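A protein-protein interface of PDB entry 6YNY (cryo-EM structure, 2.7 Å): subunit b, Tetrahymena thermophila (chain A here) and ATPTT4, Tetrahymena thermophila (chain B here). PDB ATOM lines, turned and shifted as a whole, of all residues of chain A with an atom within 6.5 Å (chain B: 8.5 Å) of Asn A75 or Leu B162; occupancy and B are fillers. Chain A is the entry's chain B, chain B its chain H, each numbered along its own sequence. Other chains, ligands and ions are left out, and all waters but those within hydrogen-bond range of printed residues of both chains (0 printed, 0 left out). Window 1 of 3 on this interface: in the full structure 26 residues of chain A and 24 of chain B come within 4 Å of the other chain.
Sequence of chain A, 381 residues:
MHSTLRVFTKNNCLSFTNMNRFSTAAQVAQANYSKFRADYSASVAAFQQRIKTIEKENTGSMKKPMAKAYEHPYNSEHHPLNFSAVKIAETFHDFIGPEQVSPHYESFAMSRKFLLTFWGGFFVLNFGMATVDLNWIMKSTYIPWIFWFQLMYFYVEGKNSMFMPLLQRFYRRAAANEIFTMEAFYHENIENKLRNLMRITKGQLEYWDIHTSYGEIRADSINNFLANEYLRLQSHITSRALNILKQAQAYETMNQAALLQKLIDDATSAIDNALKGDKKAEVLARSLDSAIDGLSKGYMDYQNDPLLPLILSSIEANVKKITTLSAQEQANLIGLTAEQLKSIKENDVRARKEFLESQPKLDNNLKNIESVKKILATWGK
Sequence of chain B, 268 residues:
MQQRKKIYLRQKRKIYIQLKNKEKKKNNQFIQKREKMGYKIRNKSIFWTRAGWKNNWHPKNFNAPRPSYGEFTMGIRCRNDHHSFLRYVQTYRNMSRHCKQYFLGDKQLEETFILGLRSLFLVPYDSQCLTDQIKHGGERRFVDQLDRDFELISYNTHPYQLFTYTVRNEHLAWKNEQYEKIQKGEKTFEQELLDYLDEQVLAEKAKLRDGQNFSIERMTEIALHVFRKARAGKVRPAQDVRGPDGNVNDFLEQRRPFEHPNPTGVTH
Among the printed residues, pairs that only touch across the chains: His A72 with Leu B162 (3.3 Å), Asn A75 with Leu B162 (3.6 Å), Leu A81 with Thr B157 (3.9 Å), Asn A82 with Pro B159 (3.8 Å) and Asn A82 with Leu B162 (3.5 Å).
Hydrophobic or aromatic side chains of chain A that line the printed part of chain B: His A72 and Leu A81. Along chain A the printed residues that touch a printed residue of chain B span positions 72 to 82. Of the 19 printed residues of chain B, 4 touch a printed residue of chain A. Printed residues of chain B that touch a printed residue of chain A: Asn B156, Thr B157, Pro B159 and Leu B162. Among the printed residues, 7 pairs touch across the chains.
A ring nitrogen (NE2) of His A72 sits at hydrogen-bond distance from the backbone carbonyl oxygen (O) of Asn B156 (2.8 Å). The side-chain amide nitrogen (ND2) of Asn A82 is in hydrogen-bond range of the backbone carbonyl oxygen (O) of Thr B157, 3.0 Å away.
The side-chain amide oxygen (OD1) of Asn B156 lies within hydrogen-bond range of the side-chain hydroxyl (OH) of Tyr B165. O of Leu B162 is in hydrogen-bond range of OG1 of Thr B166. OD1 of Asn B156 sits at hydrogen-bond distance from NE2 of Gln B161 (3.3 Å). OD1 of Asn A75 lies within hydrogen-bond range of N of Leu A81 (2.9 Å). The backbone NH (N) of Thr B157 sits at hydrogen-bond distance from the side-chain amide oxygen (OE1) of Gln B161 (3.2 Å). A ring nitrogen (ND1) of His A72 lies within hydrogen-bond range of the backbone NH of Tyr A74, at 3.1 Å.
Of the printed residues of chain B, His A72 touches Asn B156 (2.8 Å) and Leu B162 (3.3 Å). Asn A75 touches just one residue of chain B: Leu B162 (3.6 Å). No residue of chain B comes within 4 Å of Ser A76. Printed residues of chain B within 4 Å of Leu A81: Thr B157. Printed residues of chain B within 4 Å of Asn A82: Thr B157, Pro B159 and Leu B162. Printed residues of chain A within 4 Å of Thr B157: Leu A81 (3.9 Å) and Asn A82 (3.0 Å). Of the printed residues of chain A, Pro B159 touches Asn A82. Gln B161 touches none of the printed residues of chain A. Leu B162 touches three residues of chain A. The nearest residue of chain B that does not touch Asn A75 is Thr B166 (5.2 Å). The nearest residue of chain A that does not touch Leu B162 is Leu A81 (4.4 Å). The nearest printed residue of chain A that does not touch Thr B157 is His A72 (4.9 Å).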
ATOM      1  N   HIS A  72       6.538  23.447  -8.135  1.00  0.00           N
ATOM      2  CA  HIS A  72       5.969  22.816  -9.316  1.00  0.00           C
ATOM      3  C   HIS A  72       4.486  23.156  -9.421  1.00  0.00           C
ATOM      4  O   HIS A  72       3.739  22.951  -8.459  1.00  0.00           O
ATOM      5  CB  HIS A  72       6.162  21.308  -9.255  1.00  0.00           C
ATOM      6  CG  HIS A  72       6.108  20.643 -10.593  1.00  0.00           C
ATOM      7  ND1 HIS A  72       4.923  20.364 -11.236  1.00  0.00           N
ATOM      8  CD2 HIS A  72       7.093  20.202 -11.409  1.00  0.00           C
ATOM      9  CE1 HIS A  72       5.180  19.782 -12.393  1.00  0.00           C
ATOM     10  NE2 HIS A  72       6.489  19.671 -12.521  1.00  0.00           N
ATOM     11  N   PRO A  73       4.021  23.672 -10.562  1.00  0.00           N
ATOM     12  CA  PRO A  73       2.620  24.085 -10.674  1.00  0.00           C
ATOM     13  C   PRO A  73       1.646  22.967 -11.003  1.00  0.00           C
ATOM     14  O   PRO A  73       0.454  23.246 -11.167  1.00  0.00           O
ATOM     15  CB  PRO A  73       2.673  25.108 -11.812  1.00  0.00           C
ATOM     16  CG  PRO A  73       3.754  24.624 -12.675  1.00  0.00           C
ATOM     17  CD  PRO A  73       4.780  24.000 -11.779  1.00  0.00           C
ATOM     18  N   TYR A  74       2.102  21.719 -11.107  1.00  0.00           N
ATOM     19  CA  TYR A  74       1.235  20.604 -11.467  1.00  0.00           C
ATOM     20  C   TYR A  74       1.464  19.398 -10.566  1.00  0.00           C
ATOM     21  O   TYR A  74       1.197  18.262 -10.961  1.00  0.00           O
ATOM     22  CB  TYR A  74       1.422  20.221 -12.933  1.00  0.00           C
ATOM     23  CG  TYR A  74       0.848  21.230 -13.891  1.00  0.00           C
ATOM     24  CD1 TYR A  74      -0.516  21.294 -14.115  1.00  0.00           C
ATOM     25  CD2 TYR A  74       1.663  22.117 -14.571  1.00  0.00           C
ATOM     26  CE1 TYR A  74      -1.051  22.212 -14.981  1.00  0.00           C
ATOM     27  CE2 TYR A  74       1.134  23.041 -15.440  1.00  0.00           C
ATOM     28  CZ  TYR A  74      -0.224  23.083 -15.645  1.00  0.00           C
ATOM     29  OH  TYR A  74      -0.764  24.000 -16.515  1.00  0.00           O
ATOM     30  N   ASN A  75       1.955  19.627  -9.353  1.00  0.00           N
ATOM     31  CA  ASN A  75       2.134  18.563  -8.377  1.00  0.00           C
ATOM     32  C   ASN A  75       1.630  19.053  -7.031  1.00  0.00           C
ATOM     33  O   ASN A  75       2.006  20.140  -6.584  1.00  0.00           O
ATOM     34  CB  ASN A  75       3.597  18.133  -8.270  1.00  0.00           C
ATOM     35  CG  ASN A  75       3.788  16.959  -7.343  1.00  0.00           C
ATOM     36  OD1 ASN A  75       2.962  16.050  -7.295  1.00  0.00           O
ATOM     37  ND2 ASN A  75       4.877  16.974  -6.594  1.00  0.00           N
ATOM     38  N   SER A  76       0.776  18.256  -6.395  1.00  0.00           N
ATOM     39  CA  SER A  76       0.247  18.576  -5.080  1.00  0.00           C
ATOM     40  C   SER A  76       0.221  17.313  -4.236  1.00  0.00           C
ATOM     41  O   SER A  76       0.489  16.209  -4.716  1.00  0.00           O
ATOM     42  CB  SER A  76      -1.154  19.186  -5.170  1.00  0.00           C
ATOM     43  OG  SER A  76      -2.087  18.260  -5.689  1.00  0.00           O
ATOM     44  N   GLU A  77      -0.104  17.489  -2.956  1.00  0.00           N
ATOM     45  CA  GLU A  77      -0.117  16.362  -2.032  1.00  0.00           C
ATOM     46  C   GLU A  77      -1.342  15.482  -2.248  1.00  0.00           C
ATOM     47  O   GLU A  77      -1.254  14.255  -2.128  1.00  0.00           O
ATOM     48  CB  GLU A  77      -0.063  16.872  -0.593  1.00  0.00           C
ATOM     49  CG  GLU A  77       0.142  15.786   0.443  1.00  0.00           C
ATOM     50  CD  GLU A  77       0.357  16.343   1.837  1.00  0.00           C
ATOM     51  OE1 GLU A  77       0.149  17.558   2.030  1.00  0.00           O
ATOM     52  OE2 GLU A  77       0.741  15.567   2.738  1.00  0.00           O
ATOM     53  N   HIS A  79      -3.207  15.569  -5.184  1.00  0.00           N
ATOM     54  CA  HIS A  79      -3.180  15.190  -6.592  1.00  0.00           C
ATOM     55  C   HIS A  79      -1.728  15.069  -7.041  1.00  0.00           C
ATOM     56  O   HIS A  79      -1.251  15.862  -7.863  1.00  0.00           O
ATOM     57  CB  HIS A  79      -3.920  16.204  -7.459  1.00  0.00           C
ATOM     58  CG  HIS A  79      -5.398  16.228  -7.239  1.00  0.00           C
ATOM     59  ND1 HIS A  79      -6.265  15.426  -7.947  1.00  0.00           N
ATOM     60  CD2 HIS A  79      -6.164  16.967  -6.404  1.00  0.00           C
ATOM     61  CE1 HIS A  79      -7.501  15.665  -7.551  1.00  0.00           C
ATOM     62  NE2 HIS A  79      -7.467  16.594  -6.615  1.00  0.00           N
ATOM     63  N   PRO A  80      -0.997  14.087  -6.520  1.00  0.00           N
ATOM     64  CA  PRO A  80       0.399  13.922  -6.929  1.00  0.00           C
ATOM     65  C   PRO A  80       0.515  13.630  -8.415  1.00  0.00           C
ATOM     66  O   PRO A  80      -0.293  12.902  -8.993  1.00  0.00           O
ATOM     67  CB  PRO A  80       0.881  12.744  -6.078  1.00  0.00           C
ATOM     68  CG  PRO A  80      -0.340  12.082  -5.599  1.00  0.00           C
ATOM     69  CD  PRO A  80      -1.375  13.124  -5.478  1.00  0.00           C
ATOM     70  N   LEU A  81       1.544  14.212  -9.031  1.00  0.00           N
ATOM     71  CA  LEU A  81       1.708  14.080 -10.473  1.00  0.00           C
ATOM     72  C   LEU A  81       2.085  12.660 -10.863  1.00  0.00           C
ATOM     73  O   LEU A  81       1.557  12.119 -11.841  1.00  0.00           O
ATOM     74  CB  LEU A  81       2.766  15.064 -10.959  1.00  0.00           C
ATOM     75  CG  LEU A  81       3.065  15.057 -12.452  1.00  0.00           C
ATOM     76  CD1 LEU A  81       1.810  15.299 -13.256  1.00  0.00           C
ATOM     77  CD2 LEU A  81       4.092  16.104 -12.752  1.00  0.00           C
ATOM     78  N   ASN A  82       2.990  12.043 -10.117  1.00  0.00           N
ATOM     79  CA  ASN A  82       3.469  10.704 -10.406  1.00  0.00           C
ATOM     80  C   ASN A  82       2.744   9.676  -9.548  1.00  0.00           C
ATOM     81  O   ASN A  82       2.107  10.003  -8.544  1.00  0.00           O
ATOM     82  CB  ASN A  82       4.979  10.626 -10.192  1.00  0.00           C
ATOM     83  CG  ASN A  82       5.739  11.497 -11.161  1.00  0.00           C
ATOM     84  OD1 ASN A  82       5.532  11.421 -12.370  1.00  0.00           O
ATOM     85  ND2 ASN A  82       6.607  12.349 -10.638  1.00  0.00           N
ATOM     86  N   CYS B  99      18.276  19.732 -15.248  1.00  0.00           N
ATOM     87  CA  CYS B  99      17.755  19.827 -13.891  1.00  0.00           C
ATOM     88  C   CYS B  99      18.161  21.129 -13.215  1.00  0.00           C
ATOM     89  O   CYS B  99      17.431  21.624 -12.350  1.00  0.00           O
ATOM     90  CB  CYS B  99      18.229  18.638 -13.060  1.00  0.00           C
ATOM     91  SG  CYS B  99      17.397  17.089 -13.425  1.00  0.00           S
ATOM     92  N   PHE B 103      16.817  25.091 -10.327  1.00  0.00           N
ATOM     93  CA  PHE B 103      17.469  25.287  -9.041  1.00  0.00           C
ATOM     94  C   PHE B 103      17.602  26.753  -8.662  1.00  0.00           C
ATOM     95  O   PHE B 103      17.926  27.049  -7.509  1.00  0.00           O
ATOM     96  CB  PHE B 103      18.855  24.637  -9.045  1.00  0.00           C
ATOM     97  CG  PHE B 103      18.829  23.139  -9.158  1.00  0.00           C
ATOM     98  CD1 PHE B 103      17.653  22.430  -9.001  1.00  0.00           C
ATOM     99  CD2 PHE B 103      19.988  22.441  -9.420  1.00  0.00           C
ATOM    100  CE1 PHE B 103      17.639  21.064  -9.105  1.00  0.00           C
ATOM    101  CE2 PHE B 103      19.975  21.075  -9.525  1.00  0.00           C
ATOM    102  CZ  PHE B 103      18.799  20.386  -9.368  1.00  0.00           C
ATOM    103  N   LEU B 152      11.944  12.125 -18.745  1.00  0.00           N
ATOM    104  CA  LEU B 152      11.117  12.717 -17.704  1.00  0.00           C
ATOM    105  C   LEU B 152      11.731  14.001 -17.166  1.00  0.00           C
ATOM    106  O   LEU B 152      11.004  14.923 -16.785  1.00  0.00           O
ATOM    107  CB  LEU B 152      10.916  11.716 -16.570  1.00  0.00           C
ATOM    108  CG  LEU B 152      10.361  10.351 -16.962  1.00  0.00           C
ATOM    109  CD1 LEU B 152      10.353   9.432 -15.768  1.00  0.00           C
ATOM    110  CD2 LEU B 152       8.978  10.488 -17.530  1.00  0.00           C
ATOM    111  N   TYR B 155      10.920  17.137 -19.186  1.00  0.00           N
ATOM    112  CA  TYR B 155       9.594  17.671 -18.918  1.00  0.00           C
ATOM    113  C   TYR B 155       9.426  18.145 -17.483  1.00  0.00           C
ATOM    114  O   TYR B 155       8.356  18.651 -17.135  1.00  0.00           O
ATOM    115  CB  TYR B 155       8.529  16.621 -19.230  1.00  0.00           C
ATOM    116  CG  TYR B 155       8.346  16.344 -20.700  1.00  0.00           C
ATOM    117  CD1 TYR B 155       9.066  15.351 -21.335  1.00  0.00           C
ATOM    118  CD2 TYR B 155       7.447  17.075 -21.450  1.00  0.00           C
ATOM    119  CE1 TYR B 155       8.901  15.099 -22.673  1.00  0.00           C
ATOM    120  CE2 TYR B 155       7.274  16.830 -22.787  1.00  0.00           C
ATOM    121  CZ  TYR B 155       8.003  15.841 -23.394  1.00  0.00           C
ATOM    122  OH  TYR B 155       7.834  15.592 -24.732  1.00  0.00           O
ATOM    123  N   ASN B 156      10.452  18.002 -16.649  1.00  0.00           N
ATOM    124  CA  ASN B 156      10.378  18.372 -15.240  1.00  0.00           C
ATOM    125  C   ASN B 156       9.264  17.608 -14.532  1.00  0.00           C
ATOM    126  O   ASN B 156       8.443  18.178 -13.814  1.00  0.00           O
ATOM    127  CB  ASN B 156      10.196  19.879 -15.078  1.00  0.00           C
ATOM    128  CG  ASN B 156      10.452  20.344 -13.670  1.00  0.00           C
ATOM    129  OD1 ASN B 156      11.254  19.758 -12.946  1.00  0.00           O
ATOM    130  ND2 ASN B 156       9.767  21.400 -13.266  1.00  0.00           N
ATOM    131  N   THR B 157       9.236  16.293 -14.752  1.00  0.00           N
ATOM    132  CA  THR B 157       8.247  15.425 -14.129  1.00  0.00           C
ATOM    133  C   THR B 157       8.885  14.239 -13.420  1.00  0.00           C
ATOM    134  O   THR B 157       8.163  13.351 -12.957  1.00  0.00           O
ATOM    135  CB  THR B 157       7.243  14.915 -15.167  1.00  0.00           C
ATOM    136  OG1 THR B 157       7.927  14.160 -16.172  1.00  0.00           O
ATOM    137  CG2 THR B 157       6.512  16.068 -15.817  1.00  0.00           C
ATOM    138  N   HIS B 158      10.206  14.198 -13.325  1.00  0.00           N
ATOM    139  CA  HIS B 158      10.861  13.070 -12.691  1.00  0.00           C
ATOM    140  C   HIS B 158      10.666  13.140 -11.177  1.00  0.00           C
ATOM    141  O   HIS B 158      10.773  14.218 -10.587  1.00  0.00           O
ATOM    142  CB  HIS B 158      12.345  13.057 -13.029  1.00  0.00           C
ATOM    143  CG  HIS B 158      13.008  11.739 -12.798  1.00  0.00           C
ATOM    144  ND1 HIS B 158      13.344  11.285 -11.543  1.00  0.00           N
ATOM    145  CD2 HIS B 158      13.403  10.777 -13.663  1.00  0.00           C
ATOM    146  CE1 HIS B 158      13.912  10.098 -11.645  1.00  0.00           C
ATOM    147  NE2 HIS B 158      13.961   9.768 -12.922  1.00  0.00           N
ATOM    148  N   PRO B 159      10.376  12.014 -10.523  1.00  0.00           N
ATOM    149  CA  PRO B 159      10.169  12.054  -9.068  1.00  0.00           C
ATOM    150  C   PRO B 159      11.352  12.593  -8.285  1.00  0.00           C
ATOM    151  O   PRO B 159      11.149  13.207  -7.231  1.00  0.00           O
ATOM    152  CB  PRO B 159       9.874  10.590  -8.719  1.00  0.00           C
ATOM    153  CG  PRO B 159      10.250   9.805  -9.910  1.00  0.00           C
ATOM    154  CD  PRO B 159      10.075  10.687 -11.073  1.00  0.00           C
ATOM    155  N   TYR B 160      12.582  12.382  -8.753  1.00  0.00           N
ATOM    156  CA  TYR B 160      13.736  12.930  -8.051  1.00  0.00           C
ATOM    157  C   TYR B 160      13.742  14.450  -8.093  1.00  0.00           C
ATOM    158  O   TYR B 160      14.224  15.093  -7.155  1.00  0.00           O
ATOM    159  CB  TYR B 160      15.033  12.387  -8.647  1.00  0.00           C
ATOM    160  CG  TYR B 160      15.248  10.903  -8.471  1.00  0.00           C
ATOM    161  CD1 TYR B 160      14.444  10.153  -7.629  1.00  0.00           C
ATOM    162  CD2 TYR B 160      16.266  10.255  -9.145  1.00  0.00           C
ATOM    163  CE1 TYR B 160      14.645   8.806  -7.471  1.00  0.00           C
ATOM    164  CE2 TYR B 160      16.474   8.907  -8.991  1.00  0.00           C
ATOM    165  CZ  TYR B 160      15.662   8.186  -8.154  1.00  0.00           C
ATOM    166  OH  TYR B 160      15.867   6.838  -7.998  1.00  0.00           O
ATOM    167  N   GLN B 161      13.221  15.038  -9.168  1.00  0.00           N
ATOM    168  CA  GLN B 161      13.102  16.488  -9.243  1.00  0.00           C
ATOM    169  C   GLN B 161      12.093  17.009  -8.230  1.00  0.00           C
ATOM    170  O   GLN B 161      12.399  17.900  -7.432  1.00  0.00           O
ATOM    171  CB  GLN B 161      12.691  16.899 -10.653  1.00  0.00           C
ATOM    172  CG  GLN B 161      13.666  16.510 -11.733  1.00  0.00           C
ATOM    173  CD  GLN B 161      13.134  16.795 -13.116  1.00  0.00           C
ATOM    174  OE1 GLN B 161      12.164  16.187 -13.560  1.00  0.00           O
ATOM    175  NE2 GLN B 161      13.764  17.728 -13.804  1.00  0.00           N
ATOM    176  N   LEU B 162      10.879  16.462  -8.253  1.00  0.00           N
ATOM    177  CA  LEU B 162       9.847  16.902  -7.322  1.00  0.00           C
ATOM    178  C   LEU B 162      10.257  16.638  -5.883  1.00  0.00           C
ATOM    179  O   LEU B 162       9.969  17.440  -4.988  1.00  0.00           O
ATOM    180  CB  LEU B 162       8.534  16.196  -7.640  1.00  0.00           C
ATOM    181  CG  LEU B 162       8.127  16.151  -9.109  1.00  0.00           C
ATOM    182  CD1 LEU B 162       6.758  15.545  -9.246  1.00  0.00           C
ATOM    183  CD2 LEU B 162       8.155  17.515  -9.716  1.00  0.00           C
ATOM    184  N   PHE B 163      10.924  15.513  -5.641  1.00  0.00           N
ATOM    185  CA  PHE B 163      11.455  15.232  -4.315  1.00  0.00           C
ATOM    186  C   PHE B 163      12.482  16.276  -3.906  1.00  0.00           C
ATOM    187  O   PHE B 163      12.568  16.647  -2.730  1.00  0.00           O
ATOM    188  CB  PHE B 163      12.065  13.834  -4.311  1.00  0.00           C
ATOM    189  CG  PHE B 163      12.620  13.405  -2.995  1.00  0.00           C
ATOM    190  CD1 PHE B 163      11.785  13.082  -1.947  1.00  0.00           C
ATOM    191  CD2 PHE B 163      13.985  13.294  -2.814  1.00  0.00           C
ATOM    192  CE1 PHE B 163      12.298  12.675  -0.743  1.00  0.00           C
ATOM    193  CE2 PHE B 163      14.500  12.885  -1.609  1.00  0.00           C
ATOM    194  CZ  PHE B 163      13.655  12.575  -0.575  1.00  0.00           C
ATOM    195  N   THR B 164      13.258  16.773  -4.867  1.00  0.00           N
ATOM    196  CA  THR B 164      14.271  17.777  -4.565  1.00  0.00           C
ATOM    197  C   THR B 164      13.639  19.120  -4.227  1.00  0.00           C
ATOM    198  O   THR B 164      14.045  19.777  -3.263  1.00  0.00           O
ATOM    199  CB  THR B 164      15.226  17.913  -5.749  1.00  0.00           C
ATOM    200  OG1 THR B 164      15.947  16.690  -5.925  1.00  0.00           O
ATOM    201  CG2 THR B 164      16.199  19.039  -5.531  1.00  0.00           C
ATOM    202  N   TYR B 165      12.641  19.543  -5.003  1.00  0.00           N
ATOM    203  CA  TYR B 165      11.989  20.819  -4.734  1.00  0.00           C
ATOM    204  C   TYR B 165      11.317  20.811  -3.368  1.00  0.00           C
ATOM    205  O   TYR B 165      11.438  21.773  -2.602  1.00  0.00           O
ATOM    206  CB  TYR B 165      10.965  21.125  -5.822  1.00  0.00           C
ATOM    207  CG  TYR B 165      11.497  21.023  -7.228  1.00  0.00           C
ATOM    208  CD1 TYR B 165      12.794  21.393  -7.529  1.00  0.00           C
ATOM    209  CD2 TYR B 165      10.699  20.549  -8.256  1.00  0.00           C
ATOM    210  CE1 TYR B 165      13.280  21.295  -8.808  1.00  0.00           C
ATOM    211  CE2 TYR B 165      11.177  20.451  -9.534  1.00  0.00           C
ATOM    212  CZ  TYR B 165      12.467  20.822  -9.808  1.00  0.00           C
ATOM    213  OH  TYR B 165      12.939  20.719 -11.090  1.00  0.00           O
ATOM    214  N   THR B 166      10.604  19.732  -3.049  1.00  0.00           N
ATOM    215  CA  THR B 166       9.927  19.643  -1.762  1.00  0.00           C
ATOM    216  C   THR B 166      10.923  19.628  -0.612  1.00  0.00           C
ATOM    217  O   THR B 166      10.740  20.331   0.388  1.00  0.00           O
ATOM    218  CB  THR B 166       9.052  18.392  -1.727  1.00  0.00           C
ATOM    219  OG1 THR B 166       8.040  18.483  -2.735  1.00  0.00           O
ATOM    220  CG2 THR B 166       8.401  18.225  -0.376  1.00  0.00           C
ATOM    221  N   VAL B 167      11.987  18.838  -0.739  1.00  0.00           N
ATOM    222  CA  VAL B 167      12.972  18.738   0.333  1.00  0.00           C
ATOM    223  C   VAL B 167      13.677  20.070   0.542  1.00  0.00           C
ATOM    224  O   VAL B 167      13.993  20.450   1.675  1.00  0.00           O
ATOM    225  CB  VAL B 167      13.973  17.610   0.023  1.00  0.00           C
ATOM    226  CG1 VAL B 167      15.173  17.704   0.922  1.00  0.00           C
ATOM    227  CG2 VAL B 167      13.309  16.263   0.181  1.00  0.00           C
ATOM    228  N   ARG B 168      13.934  20.800  -0.542  1.00  0.00           N
ATOM    229  CA  ARG B 168      14.658  22.058  -0.418  1.00  0.00           C
ATOM    230  C   ARG B 168      13.780  23.144   0.192  1.00  0.00           C
ATOM    231  O   ARG B 168      14.232  23.895   1.064  1.00  0.00           O
ATOM    232  CB  ARG B 168      15.186  22.490  -1.783  1.00  0.00           C
ATOM    233  CG  ARG B 168      16.193  23.618  -1.740  1.00  0.00           C
ATOM    234  CD  ARG B 168      17.436  23.215  -0.989  1.00  0.00           C
ATOM    235  NE  ARG B 168      18.494  24.209  -1.081  1.00  0.00           N
ATOM    236  CZ  ARG B 168      19.608  24.171  -0.361  1.00  0.00           C
ATOM    237  NH1 ARG B 168      19.807  23.193   0.506  1.00  0.00           N
ATOM    238  NH2 ARG B 168      20.523  25.112  -0.505  1.00  0.00           N
ATOM    239  N   ASN B 169      12.529  23.246  -0.253  1.00  0.00           N
ATOM    240  CA  ASN B 169      11.625  24.236   0.321  1.00  0.00           C
ATOM    241  C   ASN B 169      11.427  24.004   1.812  1.00  0.00           C
ATOM    242  O   ASN B 169      11.356  24.960   2.592  1.00  0.00           O
ATOM    243  CB  ASN B 169      10.287  24.206  -0.411  1.00  0.00           C
ATOM    244  CG  ASN B 169      10.326  24.959  -1.717  1.00  0.00           C
ATOM    245  OD1 ASN B 169      10.958  26.005  -1.824  1.00  0.00           O
ATOM    246  ND2 ASN B 169       9.649  24.426  -2.721  1.00  0.00           N
ATOM    247  N   GLU B 170      11.333  22.741   2.231  1.00  0.00           N
ATOM    248  CA  GLU B 170      11.233  22.447   3.654  1.00  0.00           C
ATOM    249  C   GLU B 170      12.504  22.837   4.393  1.00  0.00           C
ATOM    250  O   GLU B 170      12.455  23.149   5.589  1.00  0.00           O
ATOM    251  CB  GLU B 170      10.936  20.965   3.865  1.00  0.00           C
ATOM    252  CG  GLU B 170       9.591  20.521   3.341  1.00  0.00           C
ATOM    253  CD  GLU B 170       9.412  19.017   3.376  1.00  0.00           C
ATOM    254  OE1 GLU B 170      10.377  18.308   3.731  1.00  0.00           O
ATOM    255  OE2 GLU B 170       8.303  18.541   3.053  1.00  0.00           O
